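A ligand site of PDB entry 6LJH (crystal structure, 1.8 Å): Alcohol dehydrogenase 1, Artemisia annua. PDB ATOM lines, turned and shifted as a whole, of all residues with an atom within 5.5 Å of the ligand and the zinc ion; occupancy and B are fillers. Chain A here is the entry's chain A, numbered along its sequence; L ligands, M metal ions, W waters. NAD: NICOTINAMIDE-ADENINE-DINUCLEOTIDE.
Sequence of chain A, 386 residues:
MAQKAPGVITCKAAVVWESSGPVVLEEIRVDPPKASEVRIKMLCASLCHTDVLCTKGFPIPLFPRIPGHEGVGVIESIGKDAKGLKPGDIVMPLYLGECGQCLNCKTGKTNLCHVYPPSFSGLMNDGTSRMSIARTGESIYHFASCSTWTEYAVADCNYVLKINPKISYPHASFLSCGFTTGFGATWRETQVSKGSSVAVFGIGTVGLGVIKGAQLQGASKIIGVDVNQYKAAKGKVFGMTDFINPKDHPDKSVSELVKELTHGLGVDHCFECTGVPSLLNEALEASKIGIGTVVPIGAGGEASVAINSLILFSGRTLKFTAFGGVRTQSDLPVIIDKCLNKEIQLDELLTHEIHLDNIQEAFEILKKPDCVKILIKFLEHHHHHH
Four residues have an atom within 4 Å of the zinc ion: Cys 48, His 69, Glu 70 and Cys 177.
The nearest printed residue that does not touch the zinc ion is Gly 178 (4.8 Å).
The zinc ion is bound by the side-chain carboxylate of Glu 70 (2.0 Å), a ring nitrogen (NE2) of His 69 (2.0 Å), the side-chain sulfur of Cys 48 (2.3 Å) and the side-chain sulfur of Cys 177 (2.3 Å).
The backbone NH (N) of Thr 205 is in hydrogen-bond range of an oxygen (O2N) of the ligand, at 3.3 Å.
O2D of the ligand lies within hydrogen-bond range of O of Ala 299 (2.9 Å).
The backbone NH of Val 206 lies within hydrogen-bond range of an oxygen (O2N) of the ligand, at 3.1 Å.
The side-chain carboxylate of Asp 226 is in hydrogen-bond range of an oxygen (O3B) of the ligand (2.6 Å).
The backbone carbonyl oxygen of Thr 274 is in hydrogen-bond range of an oxygen (O3D) of the ligand (2.6 Å).
An oxygen (O2D) of the ligand sits at hydrogen-bond distance from the backbone NH (N) of Ala 299.
The side-chain sulfur of Cys 177 lies close to an oxygen (O7N) of the ligand.
The side-chain amino group (NZ) of Lys 231 lies within hydrogen-bond range of an oxygen (O3B) of the ligand (2.8 Å).
NZ of Lys 373 lies within salt-bridge range of OE1 of Glu 70.
The side-chain sulfur (SG) of Cys 48 sits close to the backbone NH (N) of Thr 50.
OD2 of Asp 226 lies within hydrogen-bond range of N of Asn 228, at 2.8 Å.
O of Cys 177 is in hydrogen-bond range of OG1 of Thr 181 (3.0 Å).
N of Gly 300 sits close to O of Gly 275.
The backbone NH of Cys 273 sits at hydrogen-bond distance from the backbone carbonyl oxygen of Phe 201.
N of Ile 203 sits at hydrogen-bond distance from OD1 of Asp 226 (2.8 Å).
The side-chain amino group of Lys 231 lies close to the backbone carbonyl oxygen of Ile 203.
Water W10 bridges an oxygen (O1A) of the ligand (2.6 Å) and the side-chain amino group of Lys 231 (2.6 Å).
Water W1 lies within hydrogen-bond range of O1A of the ligand (2.7 Å), O of Val 372 (2.8 Å) and N of Thr 205 (3.1 Å).
Water W2 lies within hydrogen-bond range of an oxygen (O1N) of the ligand (2.8 Å) and the side-chain amino group (NZ) of Lys 373 (3.1 Å).
Water W5 lies within hydrogen-bond range of ND2 of Asn 228 (2.8 Å), O3B of the ligand (2.8 Å) and NZ of Lys 231 (3.1 Å).
Water W3 lies within hydrogen-bond range of N of Gly 204 (2.9 Å), O2N of the ligand (2.9 Å), O of Cys 273 (3.0 Å), N of Gly 207 (3.1 Å) and O of Gly 202 (3.3 Å).
His 49 touches the ligand (CB to C6N, 3.5 Å).
OG1 of Thr 50 touches C5N of the ligand, at 3.7 Å.
CG2 of Thr 181 touches N7N of the ligand, at 3.7 Å.
Gly 202 touches the ligand.
N of Ile 203 touches C4B of the ligand, at 3.96 Å.
Gly 204 touches the ligand (CA to O5B, 3.4 Å).
Val 227 touches the ligand.
Asn 228 touches the ligand (CB to O2B, 3.8 Å).
Cys 273 touches the ligand.
Gly 275 touches the ligand (CA to O2D, 3.6 Å).
Val 276 touches the ligand.
Leu 279 touches the ligand (CD1 to N1A, 3.7 Å).
Ile 297 touches the ligand (CG2 to N7N, 3.7 Å).
Gly 298 touches the ligand.
Hydrophobic or aromatic side chains within 4 Å of the ligand: His 49, Val 206, Val 227, Val 276, Leu 279 and Ile 297.
Of the 34 residues printed, 22 come within 4 Å of the ligand.
The nearest printed residue that does not touch the ligand is Val 225 (4.03 Å).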
ATOM      1  N   LEU A  47      23.072  18.427  24.559  1.00  0.00           N
ATOM      2  CA  LEU A  47      23.791  19.678  24.744  1.00  0.00           C
ATOM      3  C   LEU A  47      23.539  20.539  23.523  1.00  0.00           C
ATOM      4  O   LEU A  47      23.533  20.036  22.392  1.00  0.00           O
ATOM      5  CB  LEU A  47      25.302  19.422  24.898  1.00  0.00           C
ATOM      6  CG  LEU A  47      26.348  20.539  24.970  1.00  0.00           C
ATOM      7  CD1 LEU A  47      27.613  20.011  25.653  1.00  0.00           C
ATOM      8  CD2 LEU A  47      26.713  21.111  23.601  1.00  0.00           C
ATOM      9  N   CYS A  48      23.350  21.834  23.735  1.00  0.00           N
ATOM     10  CA  CYS A  48      23.382  22.792  22.639  1.00  0.00           C
ATOM     11  C   CYS A  48      24.084  24.059  23.118  1.00  0.00           C
ATOM     12  O   CYS A  48      24.582  24.132  24.248  1.00  0.00           O
ATOM     13  CB  CYS A  48      21.977  23.082  22.092  1.00  0.00           C
ATOM     14  SG  CYS A  48      21.007  24.271  23.037  1.00  0.00           S
ATOM     15  N   HIS A  49      24.153  25.067  22.231  1.00  0.00           N
ATOM     16  CA  HIS A  49      24.929  26.276  22.530  1.00  0.00           C
ATOM     17  C   HIS A  49      24.421  26.973  23.787  1.00  0.00           C
ATOM     18  O   HIS A  49      25.207  27.618  24.503  1.00  0.00           O
ATOM     19  CB  HIS A  49      24.868  27.226  21.336  1.00  0.00           C
ATOM     20  CG  HIS A  49      25.684  28.465  21.531  1.00  0.00           C
ATOM     21  ND1 HIS A  49      27.060  28.448  21.605  1.00  0.00           N
ATOM     22  CD2 HIS A  49      25.313  29.769  21.673  1.00  0.00           C
ATOM     23  CE1 HIS A  49      27.501  29.679  21.779  1.00  0.00           C
ATOM     24  NE2 HIS A  49      26.467  30.499  21.820  1.00  0.00           N
ATOM     25  N   THR A  50      23.128  26.859  24.073  1.00  0.00           N
ATOM     26  CA  THR A  50      22.570  27.493  25.258  1.00  0.00           C
ATOM     27  C   THR A  50      23.236  26.973  26.535  1.00  0.00           C
ATOM     28  O   THR A  50      23.414  27.723  27.492  1.00  0.00           O
ATOM     29  CB  THR A  50      21.057  27.267  25.275  1.00  0.00           C
ATOM     30  OG1 THR A  50      20.498  27.825  24.078  1.00  0.00           O
ATOM     31  CG2 THR A  50      20.413  27.911  26.494  1.00  0.00           C
ATOM     32  N   ASP A  51      23.639  25.694  26.547  1.00  0.00           N
ATOM     33  CA  ASP A  51      24.358  25.163  27.709  1.00  0.00           C
ATOM     34  C   ASP A  51      25.760  25.744  27.794  1.00  0.00           C
ATOM     35  O   ASP A  51      26.254  26.021  28.898  1.00  0.00           O
ATOM     36  CB  ASP A  51      24.425  23.642  27.626  1.00  0.00           C
ATOM     37  CG  ASP A  51      23.064  23.002  27.619  1.00  0.00           C
ATOM     38  OD1 ASP A  51      22.279  23.312  28.533  1.00  0.00           O
ATOM     39  OD2 ASP A  51      22.766  22.213  26.699  1.00  0.00           O
ATOM     40  N   HIS A  69      19.499  21.257  29.547  1.00  0.00           N
ATOM     41  CA  HIS A  69      18.056  21.389  29.417  1.00  0.00           C
ATOM     42  C   HIS A  69      17.455  20.319  28.514  1.00  0.00           C
ATOM     43  O   HIS A  69      16.231  20.134  28.549  1.00  0.00           O
ATOM     44  CB  HIS A  69      17.699  22.776  28.854  1.00  0.00           C
ATOM     45  CG  HIS A  69      18.360  23.057  27.544  1.00  0.00           C
ATOM     46  ND1 HIS A  69      19.710  23.317  27.431  1.00  0.00           N
ATOM     47  CD2 HIS A  69      17.858  23.070  26.283  1.00  0.00           C
ATOM     48  CE1 HIS A  69      20.012  23.481  26.151  1.00  0.00           C
ATOM     49  NE2 HIS A  69      18.908  23.334  25.438  1.00  0.00           N
ATOM     50  N   GLU A  70      18.266  19.650  27.700  1.00  0.00           N
ATOM     51  CA  GLU A  70      17.796  18.638  26.768  1.00  0.00           C
ATOM     52  C   GLU A  70      17.958  17.259  27.379  1.00  0.00           C
ATOM     53  O   GLU A  70      19.026  16.907  27.878  1.00  0.00           O
ATOM     54  CB  GLU A  70      18.595  18.700  25.455  1.00  0.00           C
ATOM     55  CG  GLU A  70      18.608  20.070  24.822  1.00  0.00           C
ATOM     56  CD  GLU A  70      19.370  20.110  23.512  1.00  0.00           C
ATOM     57  OE1 GLU A  70      19.885  19.052  23.094  1.00  0.00           O
ATOM     58  OE2 GLU A  70      19.464  21.209  22.919  1.00  0.00           O
ATOM     59  N   CYS A 177      14.420  20.152  22.072  1.00  0.00           N
ATOM     60  CA  CYS A 177      14.941  21.497  21.799  1.00  0.00           C
ATOM     61  C   CYS A 177      15.048  21.813  20.297  1.00  0.00           C
ATOM     62  O   CYS A 177      14.040  22.131  19.662  1.00  0.00           O
ATOM     63  CB  CYS A 177      16.305  21.704  22.480  1.00  0.00           C
ATOM     64  SG  CYS A 177      17.001  23.412  22.355  1.00  0.00           S
ATOM     65  N   GLY A 178      16.245  21.690  19.735  1.00  0.00           N
ATOM     66  CA  GLY A 178      16.541  22.373  18.474  1.00  0.00           C
ATOM     67  C   GLY A 178      15.763  21.851  17.266  1.00  0.00           C
ATOM     68  O   GLY A 178      15.225  22.639  16.481  1.00  0.00           O
ATOM     69  N   THR A 181      12.216  22.976  17.400  1.00  0.00           N
ATOM     70  CA  THR A 181      12.150  24.408  17.141  1.00  0.00           C
ATOM     71  C   THR A 181      12.153  24.694  15.644  1.00  0.00           C
ATOM     72  O   THR A 181      11.282  25.415  15.140  1.00  0.00           O
ATOM     73  CB  THR A 181      13.325  25.101  17.841  1.00  0.00           C
ATOM     74  OG1 THR A 181      13.153  25.008  19.260  1.00  0.00           O
ATOM     75  CG2 THR A 181      13.390  26.550  17.435  1.00  0.00           C
ATOM     76  N   PHE A 201      19.484  29.298   6.859  1.00  0.00           N
ATOM     77  CA  PHE A 201      20.851  29.726   7.161  1.00  0.00           C
ATOM     78  C   PHE A 201      21.320  28.928   8.374  1.00  0.00           C
ATOM     79  O   PHE A 201      20.829  29.144   9.475  1.00  0.00           O
ATOM     80  CB  PHE A 201      20.937  31.217   7.482  1.00  0.00           C
ATOM     81  CG  PHE A 201      20.664  32.142   6.331  1.00  0.00           C
ATOM     82  CD1 PHE A 201      20.213  31.674   5.107  1.00  0.00           C
ATOM     83  CD2 PHE A 201      20.857  33.498   6.491  1.00  0.00           C
ATOM     84  CE1 PHE A 201      19.949  32.562   4.065  1.00  0.00           C
ATOM     85  CE2 PHE A 201      20.596  34.378   5.455  1.00  0.00           C
ATOM     86  CZ  PHE A 201      20.138  33.898   4.234  1.00  0.00           C
ATOM     87  N   GLY A 202      22.263  28.027   8.159  1.00  0.00           N
ATOM     88  CA  GLY A 202      22.768  27.226   9.257  1.00  0.00           C
ATOM     89  C   GLY A 202      22.088  25.882   9.289  1.00  0.00           C
ATOM     90  O   GLY A 202      20.854  25.823   9.370  1.00  0.00           O
ATOM     91  N   ILE A 203      22.872  24.799   9.210  1.00  0.00           N
ATOM     92  CA  ILE A 203      22.334  23.457   9.047  1.00  0.00           C
ATOM     93  C   ILE A 203      22.759  22.583  10.223  1.00  0.00           C
ATOM     94  O   ILE A 203      23.261  21.472  10.048  1.00  0.00           O
ATOM     95  CB  ILE A 203      22.777  22.851   7.697  1.00  0.00           C
ATOM     96  CG1 ILE A 203      22.574  23.840   6.554  1.00  0.00           C
ATOM     97  CG2 ILE A 203      21.962  21.628   7.358  1.00  0.00           C
ATOM     98  CD1 ILE A 203      22.834  23.238   5.185  1.00  0.00           C
ATOM     99  N   GLY A 204      22.570  23.094  11.439  1.00  0.00           N
ATOM    100  CA  GLY A 204      22.657  22.276  12.633  1.00  0.00           C
ATOM    101  C   GLY A 204      21.308  21.620  12.840  1.00  0.00           C
ATOM    102  O   GLY A 204      20.468  21.594  11.942  1.00  0.00           O
ATOM    103  N   THR A 205      21.081  21.119  14.064  1.00  0.00           N
ATOM    104  CA  THR A 205      19.825  20.443  14.345  1.00  0.00           C
ATOM    105  C   THR A 205      18.618  21.357  14.068  1.00  0.00           C
ATOM    106  O   THR A 205      17.583  20.886  13.563  1.00  0.00           O
ATOM    107  CB  THR A 205      19.814  19.914  15.780  1.00  0.00           C
ATOM    108  OG1 THR A 205      18.659  19.074  15.972  1.00  0.00           O
ATOM    109  CG2 THR A 205      19.783  21.069  16.809  1.00  0.00           C
ATOM    110  N   VAL A 206      18.746  22.658  14.343  1.00  0.00           N
ATOM    111  CA  VAL A 206      17.636  23.584  14.077  1.00  0.00           C
ATOM    112  C   VAL A 206      17.350  23.659  12.583  1.00  0.00           C
ATOM    113  O   VAL A 206      16.208  23.486  12.148  1.00  0.00           O
ATOM    114  CB  VAL A 206      17.926  24.981  14.647  1.00  0.00           C
ATOM    115  CG1 VAL A 206      16.831  25.954  14.218  1.00  0.00           C
ATOM    116  CG2 VAL A 206      18.051  24.933  16.162  1.00  0.00           C
ATOM    117  N   GLY A 207      18.381  23.951  11.789  1.00  0.00           N
ATOM    118  CA  GLY A 207      18.178  24.037  10.349  1.00  0.00           C
ATOM    119  C   GLY A 207      17.732  22.728   9.723  1.00  0.00           C
ATOM    120  O   GLY A 207      16.962  22.742   8.759  1.00  0.00           O
ATOM    121  N   VAL A 225      22.198  26.878   3.682  1.00  0.00           N
ATOM    122  CA  VAL A 225      23.407  27.696   3.655  1.00  0.00           C
ATOM    123  C   VAL A 225      24.261  27.350   4.865  1.00  0.00           C
ATOM    124  O   VAL A 225      23.792  27.453   6.009  1.00  0.00           O
ATOM    125  CB  VAL A 225      23.096  29.203   3.645  1.00  0.00           C
ATOM    126  CG1 VAL A 225      24.368  30.032   3.436  1.00  0.00           C
ATOM    127  CG2 VAL A 225      22.056  29.532   2.574  1.00  0.00           C
ATOM    128  N   ASP A 226      25.520  26.957   4.631  1.00  0.00           N
ATOM    129  CA  ASP A 226      26.421  26.671   5.740  1.00  0.00           C
ATOM    130  C   ASP A 226      27.873  26.784   5.282  1.00  0.00           C
ATOM    131  O   ASP A 226      28.201  26.377   4.157  1.00  0.00           O
ATOM    132  CB  ASP A 226      26.153  25.278   6.327  1.00  0.00           C
ATOM    133  CG  ASP A 226      26.509  25.190   7.805  1.00  0.00           C
ATOM    134  OD1 ASP A 226      25.602  24.956   8.629  1.00  0.00           O
ATOM    135  OD2 ASP A 226      27.708  25.374   8.155  1.00  0.00           O
ATOM    136  N   VAL A 227      28.718  27.337   6.150  1.00  0.00           N
ATOM    137  CA  VAL A 227      30.151  27.384   5.864  1.00  0.00           C
ATOM    138  C   VAL A 227      30.835  26.039   6.092  1.00  0.00           C
ATOM    139  O   VAL A 227      31.967  25.861   5.645  1.00  0.00           O
ATOM    140  CB  VAL A 227      30.876  28.459   6.697  1.00  0.00           C
ATOM    141  CG1 VAL A 227      30.407  29.854   6.292  1.00  0.00           C
ATOM    142  CG2 VAL A 227      30.674  28.226   8.218  1.00  0.00           C
ATOM    143  N   ASN A 228      30.158  25.100   6.753  1.00  0.00           N
ATOM    144  CA  ASN A 228      30.710  23.774   7.035  1.00  0.00           C
ATOM    145  C   ASN A 228      30.221  22.815   5.966  1.00  0.00           C
ATOM    146  O   ASN A 228      29.056  22.395   5.975  1.00  0.00           O
ATOM    147  CB  ASN A 228      30.316  23.287   8.433  1.00  0.00           C
ATOM    148  CG  ASN A 228      30.856  21.896   8.753  1.00  0.00           C
ATOM    149  OD1 ASN A 228      31.567  21.284   7.942  1.00  0.00           O
ATOM    150  ND2 ASN A 228      30.503  21.374   9.929  1.00  0.00           N
ATOM    151  N   LYS A 231      28.004  19.683   6.437  1.00  0.00           N
ATOM    152  CA  LYS A 231      26.569  19.738   6.673  1.00  0.00           C
ATOM    153  C   LYS A 231      25.744  19.493   5.417  1.00  0.00           C
ATOM    154  O   LYS A 231      24.561  19.166   5.519  1.00  0.00           O
ATOM    155  CB  LYS A 231      26.169  21.086   7.288  1.00  0.00           C
ATOM    156  CG  LYS A 231      26.640  21.289   8.739  1.00  0.00           C
ATOM    157  CD  LYS A 231      26.204  20.119   9.610  1.00  0.00           C
ATOM    158  CE  LYS A 231      26.713  20.282  11.040  1.00  0.00           C
ATOM    159  NZ  LYS A 231      26.134  21.471  11.706  1.00  0.00           N
ATOM    160  N   PRO A 246      28.929  29.893   1.824  1.00  0.00           N
ATOM    161  CA  PRO A 246      29.374  31.280   1.613  1.00  0.00           C
ATOM    162  C   PRO A 246      30.871  31.407   1.361  1.00  0.00           C
ATOM    163  O   PRO A 246      31.295  32.340   0.661  1.00  0.00           O
ATOM    164  CB  PRO A 246      28.966  31.986   2.910  1.00  0.00           C
ATOM    165  CG  PRO A 246      27.809  31.170   3.440  1.00  0.00           C
ATOM    166  CD  PRO A 246      28.132  29.741   3.057  1.00  0.00           C
ATOM    167  N   CYS A 273      19.138  30.352  11.275  1.00  0.00           N
ATOM    168  CA  CYS A 273      19.435  29.294  12.231  1.00  0.00           C
ATOM    169  C   CYS A 273      20.912  29.244  12.602  1.00  0.00           C
ATOM    170  O   CYS A 273      21.436  28.191  12.973  1.00  0.00           O
ATOM    171  CB  CYS A 273      18.988  27.931  11.694  1.00  0.00           C
ATOM    172  SG  CYS A 273      17.260  27.897  11.110  1.00  0.00           S
ATOM    173  N   THR A 274      21.614  30.380  12.471  1.00  0.00           N
ATOM    174  CA  THR A 274      22.992  30.486  12.935  1.00  0.00           C
ATOM    175  C   THR A 274      23.149  31.354  14.173  1.00  0.00           C
ATOM    176  O   THR A 274      24.059  31.126  14.971  1.00  0.00           O
ATOM    177  CB  THR A 274      23.919  31.080  11.861  1.00  0.00           C
ATOM    178  OG1 THR A 274      23.654  32.483  11.728  1.00  0.00           O
ATOM    179  CG2 THR A 274      23.731  30.387  10.508  1.00  0.00           C
ATOM    180  N   GLY A 275      22.323  32.378  14.332  1.00  0.00           N
ATOM    181  CA  GLY A 275      22.544  33.339  15.398  1.00  0.00           C
ATOM    182  C   GLY A 275      23.575  34.399  15.091  1.00  0.00           C
ATOM    183  O   GLY A 275      23.803  35.282  15.925  1.00  0.00           O
ATOM    184  N   VAL A 276      24.206  34.340  13.917  1.00  0.00           N
ATOM    185  CA  VAL A 276      25.217  35.333  13.518  1.00  0.00           C
ATOM    186  C   VAL A 276      24.507  36.665  13.282  1.00  0.00           C
ATOM    187  O   VAL A 276      23.604  36.734  12.427  1.00  0.00           O
ATOM    188  CB  VAL A 276      25.989  34.863  12.275  1.00  0.00           C
ATOM    189  CG1 VAL A 276      26.960  35.957  11.804  1.00  0.00           C
ATOM    190  CG2 VAL A 276      26.747  33.591  12.598  1.00  0.00           C
ATOM    191  N   LEU A 279      23.778  38.029   9.864  1.00  0.00           N
ATOM    192  CA  LEU A 279      22.954  37.187   8.998  1.00  0.00           C
ATOM    193  C   LEU A 279      21.461  37.452   9.149  1.00  0.00           C
ATOM    194  O   LEU A 279      20.680  36.979   8.316  1.00  0.00           O
ATOM    195  CB  LEU A 279      23.255  35.712   9.249  1.00  0.00           C
ATOM    196  CG  LEU A 279      24.562  35.218   8.617  1.00  0.00           C
ATOM    197  CD1 LEU A 279      24.740  33.714   8.788  1.00  0.00           C
ATOM    198  CD2 LEU A 279      24.626  35.606   7.131  1.00  0.00           C
ATOM    199  N   ILE A 297      15.506  32.294  14.293  1.00  0.00           N
ATOM    200  CA  ILE A 297      15.507  31.325  15.375  1.00  0.00           C
ATOM    201  C   ILE A 297      16.799  31.411  16.187  1.00  0.00           C
ATOM    202  O   ILE A 297      16.770  31.401  17.421  1.00  0.00           O
ATOM    203  CB  ILE A 297      15.299  29.911  14.797  1.00  0.00           C
ATOM    204  CG1 ILE A 297      13.942  29.798  14.087  1.00  0.00           C
ATOM    205  CG2 ILE A 297      15.434  28.874  15.901  1.00  0.00           C
ATOM    206  CD1 ILE A 297      13.776  28.472  13.304  1.00  0.00           C
ATOM    207  N   GLY A 298      17.947  31.491  15.523  1.00  0.00           N
ATOM    208  CA  GLY A 298      19.209  31.555  16.241  1.00  0.00           C
ATOM    209  C   GLY A 298      19.357  32.843  17.033  1.00  0.00           C
ATOM    210  O   GLY A 298      18.779  33.878  16.716  1.00  0.00           O
ATOM    211  N   ALA A 299      20.167  32.766  18.088  1.00  0.00           N
ATOM    212  CA  ALA A 299      20.403  33.879  19.002  1.00  0.00           C
ATOM    213  C   ALA A 299      21.883  34.221  19.010  1.00  0.00           C
ATOM    214  O   ALA A 299      22.731  33.321  19.065  1.00  0.00           O
ATOM    215  CB  ALA A 299      19.958  33.525  20.419  1.00  0.00           C
ATOM    216  N   GLY A 300      22.193  35.513  18.943  1.00  0.00           N
ATOM    217  CA  GLY A 300      23.567  35.982  18.966  1.00  0.00           C
ATOM    218  C   GLY A 300      24.103  36.388  20.319  1.00  0.00           C
ATOM    219  O   GLY A 300      25.309  36.601  20.446  1.00  0.00           O
ATOM    220  N   VAL A 372      26.976  16.716  14.890  1.00  0.00           N
ATOM    221  CA  VAL A 372      25.639  17.307  14.784  1.00  0.00           C
ATOM    222  C   VAL A 372      25.021  17.366  16.176  1.00  0.00           C
ATOM    223  O   VAL A 372      24.804  18.456  16.709  1.00  0.00           O
ATOM    224  CB  VAL A 372      24.738  16.530  13.792  1.00  0.00           C
ATOM    225  CG1 VAL A 372      23.374  17.198  13.684  1.00  0.00           C
ATOM    226  CG2 VAL A 372      25.384  16.464  12.394  1.00  0.00           C
ATOM    227  N   LYS A 373      24.753  16.211  16.786  1.00  0.00           N
ATOM    228  CA  LYS A 373      24.221  16.144  18.152  1.00  0.00           C
ATOM    229  C   LYS A 373      25.052  15.168  18.982  1.00  0.00           C
ATOM    230  O   LYS A 373      25.430  14.105  18.490  1.00  0.00           O
ATOM    231  CB  LYS A 373      22.743  15.711  18.176  1.00  0.00           C
ATOM    232  CG  LYS A 373      21.736  16.773  17.691  1.00  0.00           C
ATOM    233  CD  LYS A 373      21.824  18.084  18.488  1.00  0.00           C
ATOM    234  CE  LYS A 373      21.259  17.933  19.913  1.00  0.00           C
ATOM    235  NZ  LYS A 373      21.357  19.224  20.637  1.00  0.00           N
HETATM  236  PA  NAD L   1      24.599  24.394  15.442  1.00  0.00           P
HETATM  237  O1A NAD L   1      24.530  22.883  15.513  1.00  0.00           O
HETATM  238  O2A NAD L   1      25.891  24.986  15.970  1.00  0.00           O
HETATM  239  O5B NAD L   1      24.379  24.884  13.908  1.00  0.00           O
HETATM  240  C5B NAD L   1      24.855  26.137  13.555  1.00  0.00           C
HETATM  241  C4B NAD L   1      25.297  25.940  12.130  1.00  0.00           C
HETATM  242  O4B NAD L   1      25.462  27.385  11.522  1.00  0.00           O
HETATM  243  C3B NAD L   1      26.485  25.265  12.031  1.00  0.00           C
HETATM  244  O3B NAD L   1      26.375  24.162  11.033  1.00  0.00           O
HETATM  245  C2B NAD L   1      27.495  26.296  11.539  1.00  0.00           C
HETATM  246  O2B NAD L   1      28.425  25.766  10.675  1.00  0.00           O
HETATM  247  C1B NAD L   1      26.548  27.311  10.786  1.00  0.00           C
HETATM  248  N9A NAD L   1      27.145  28.627  10.770  1.00  0.00           N
HETATM  249  C8A NAD L   1      27.739  29.284  11.783  1.00  0.00           C
HETATM  250  N7A NAD L   1      28.145  30.498  11.310  1.00  0.00           N
HETATM  251  C5A NAD L   1      27.777  30.561  10.025  1.00  0.00           C
HETATM  252  C6A NAD L   1      27.931  31.626   8.959  1.00  0.00           C
HETATM  253  N6A NAD L   1      28.586  32.875   9.282  1.00  0.00           N
HETATM  254  N1A NAD L   1      27.414  31.393   7.671  1.00  0.00           N
HETATM  255  C2A NAD L   1      26.749  30.177   7.326  1.00  0.00           C
HETATM  256  N3A NAD L   1      26.618  29.146   8.338  1.00  0.00           N
HETATM  257  C4A NAD L   1      27.150  29.396   9.701  1.00  0.00           C
HETATM  258  O3  NAD L   1      23.468  25.131  16.341  1.00  0.00           O
HETATM  259  PN  NAD L   1      21.904  24.707  16.512  1.00  0.00           P
HETATM  260  O1N NAD L   1      21.739  23.752  17.619  1.00  0.00           O
HETATM  261  O2N NAD L   1      21.331  24.132  15.297  1.00  0.00           O
HETATM  262  O5D NAD L   1      21.200  26.129  16.896  1.00  0.00           O
HETATM  263  C5D NAD L   1      21.283  27.113  15.891  1.00  0.00           C
HETATM  264  C4D NAD L   1      21.698  28.437  16.442  1.00  0.00           C
HETATM  265  O4D NAD L   1      20.572  28.918  17.456  1.00  0.00           O
HETATM  266  C3D NAD L   1      22.866  28.424  17.144  1.00  0.00           C
HETATM  267  O3D NAD L   1      23.973  28.821  16.267  1.00  0.00           O
HETATM  268  C2D NAD L   1      22.648  29.432  18.264  1.00  0.00           C
HETATM  269  O2D NAD L   1      22.820  30.706  17.842  1.00  0.00           O
HETATM  270  C1D NAD L   1      21.116  29.352  18.549  1.00  0.00           C
HETATM  271  N1N NAD L   1      20.687  28.264  19.334  1.00  0.00           N
HETATM  272  C2N NAD L   1      19.228  28.057  19.298  1.00  0.00           C
HETATM  273  C3N NAD L   1      18.601  26.903  20.040  1.00  0.00           C
HETATM  274  C7N NAD L   1      17.100  26.755  20.001  1.00  0.00           C
HETATM  275  O7N NAD L   1      16.561  25.863  20.554  1.00  0.00           O
HETATM  276  N7N NAD L   1      16.355  27.751  19.272  1.00  0.00           N
HETATM  277  C4N NAD L   1      19.485  25.983  20.799  1.00  0.00           C
HETATM  278  C5N NAD L   1      20.966  26.224  20.782  1.00  0.00           C
HETATM  279  C6N NAD L   1      21.617  27.374  20.041  1.00  0.00           C
HETATM  280 ZN    ZN M   1      19.045  23.116  23.414  1.00  0.00          ZN
HETATM  281  O   HOH W   1      23.176  20.702  16.246  1.00  0.00           O
HETATM  282  O   HOH W   2      22.660  21.407  18.828  1.00  0.00           O
HETATM  283  O   HOH W   3      21.066  25.222  12.649  1.00  0.00           O
HETATM  284  O   HOH W   4      26.428  27.823  16.877  1.00  0.00           O
HETATM  285  O   HOH W   5      28.892  22.962  11.553  1.00  0.00           O
HETATM  286  O   HOH W   6      28.444  24.723  15.456  1.00  0.00           O
HETATM  287  O   HOH W   7      19.618  23.460  19.133  1.00  0.00           O
HETATM  288  O   HOH W   8      31.124  26.257  11.323  1.00  0.00           O
HETATM  289  O   HOH W   9      25.921  25.043  18.814  1.00  0.00           O
HETATM  290  O   HOH W  10      25.862  21.051  14.288  1.00  0.00           O
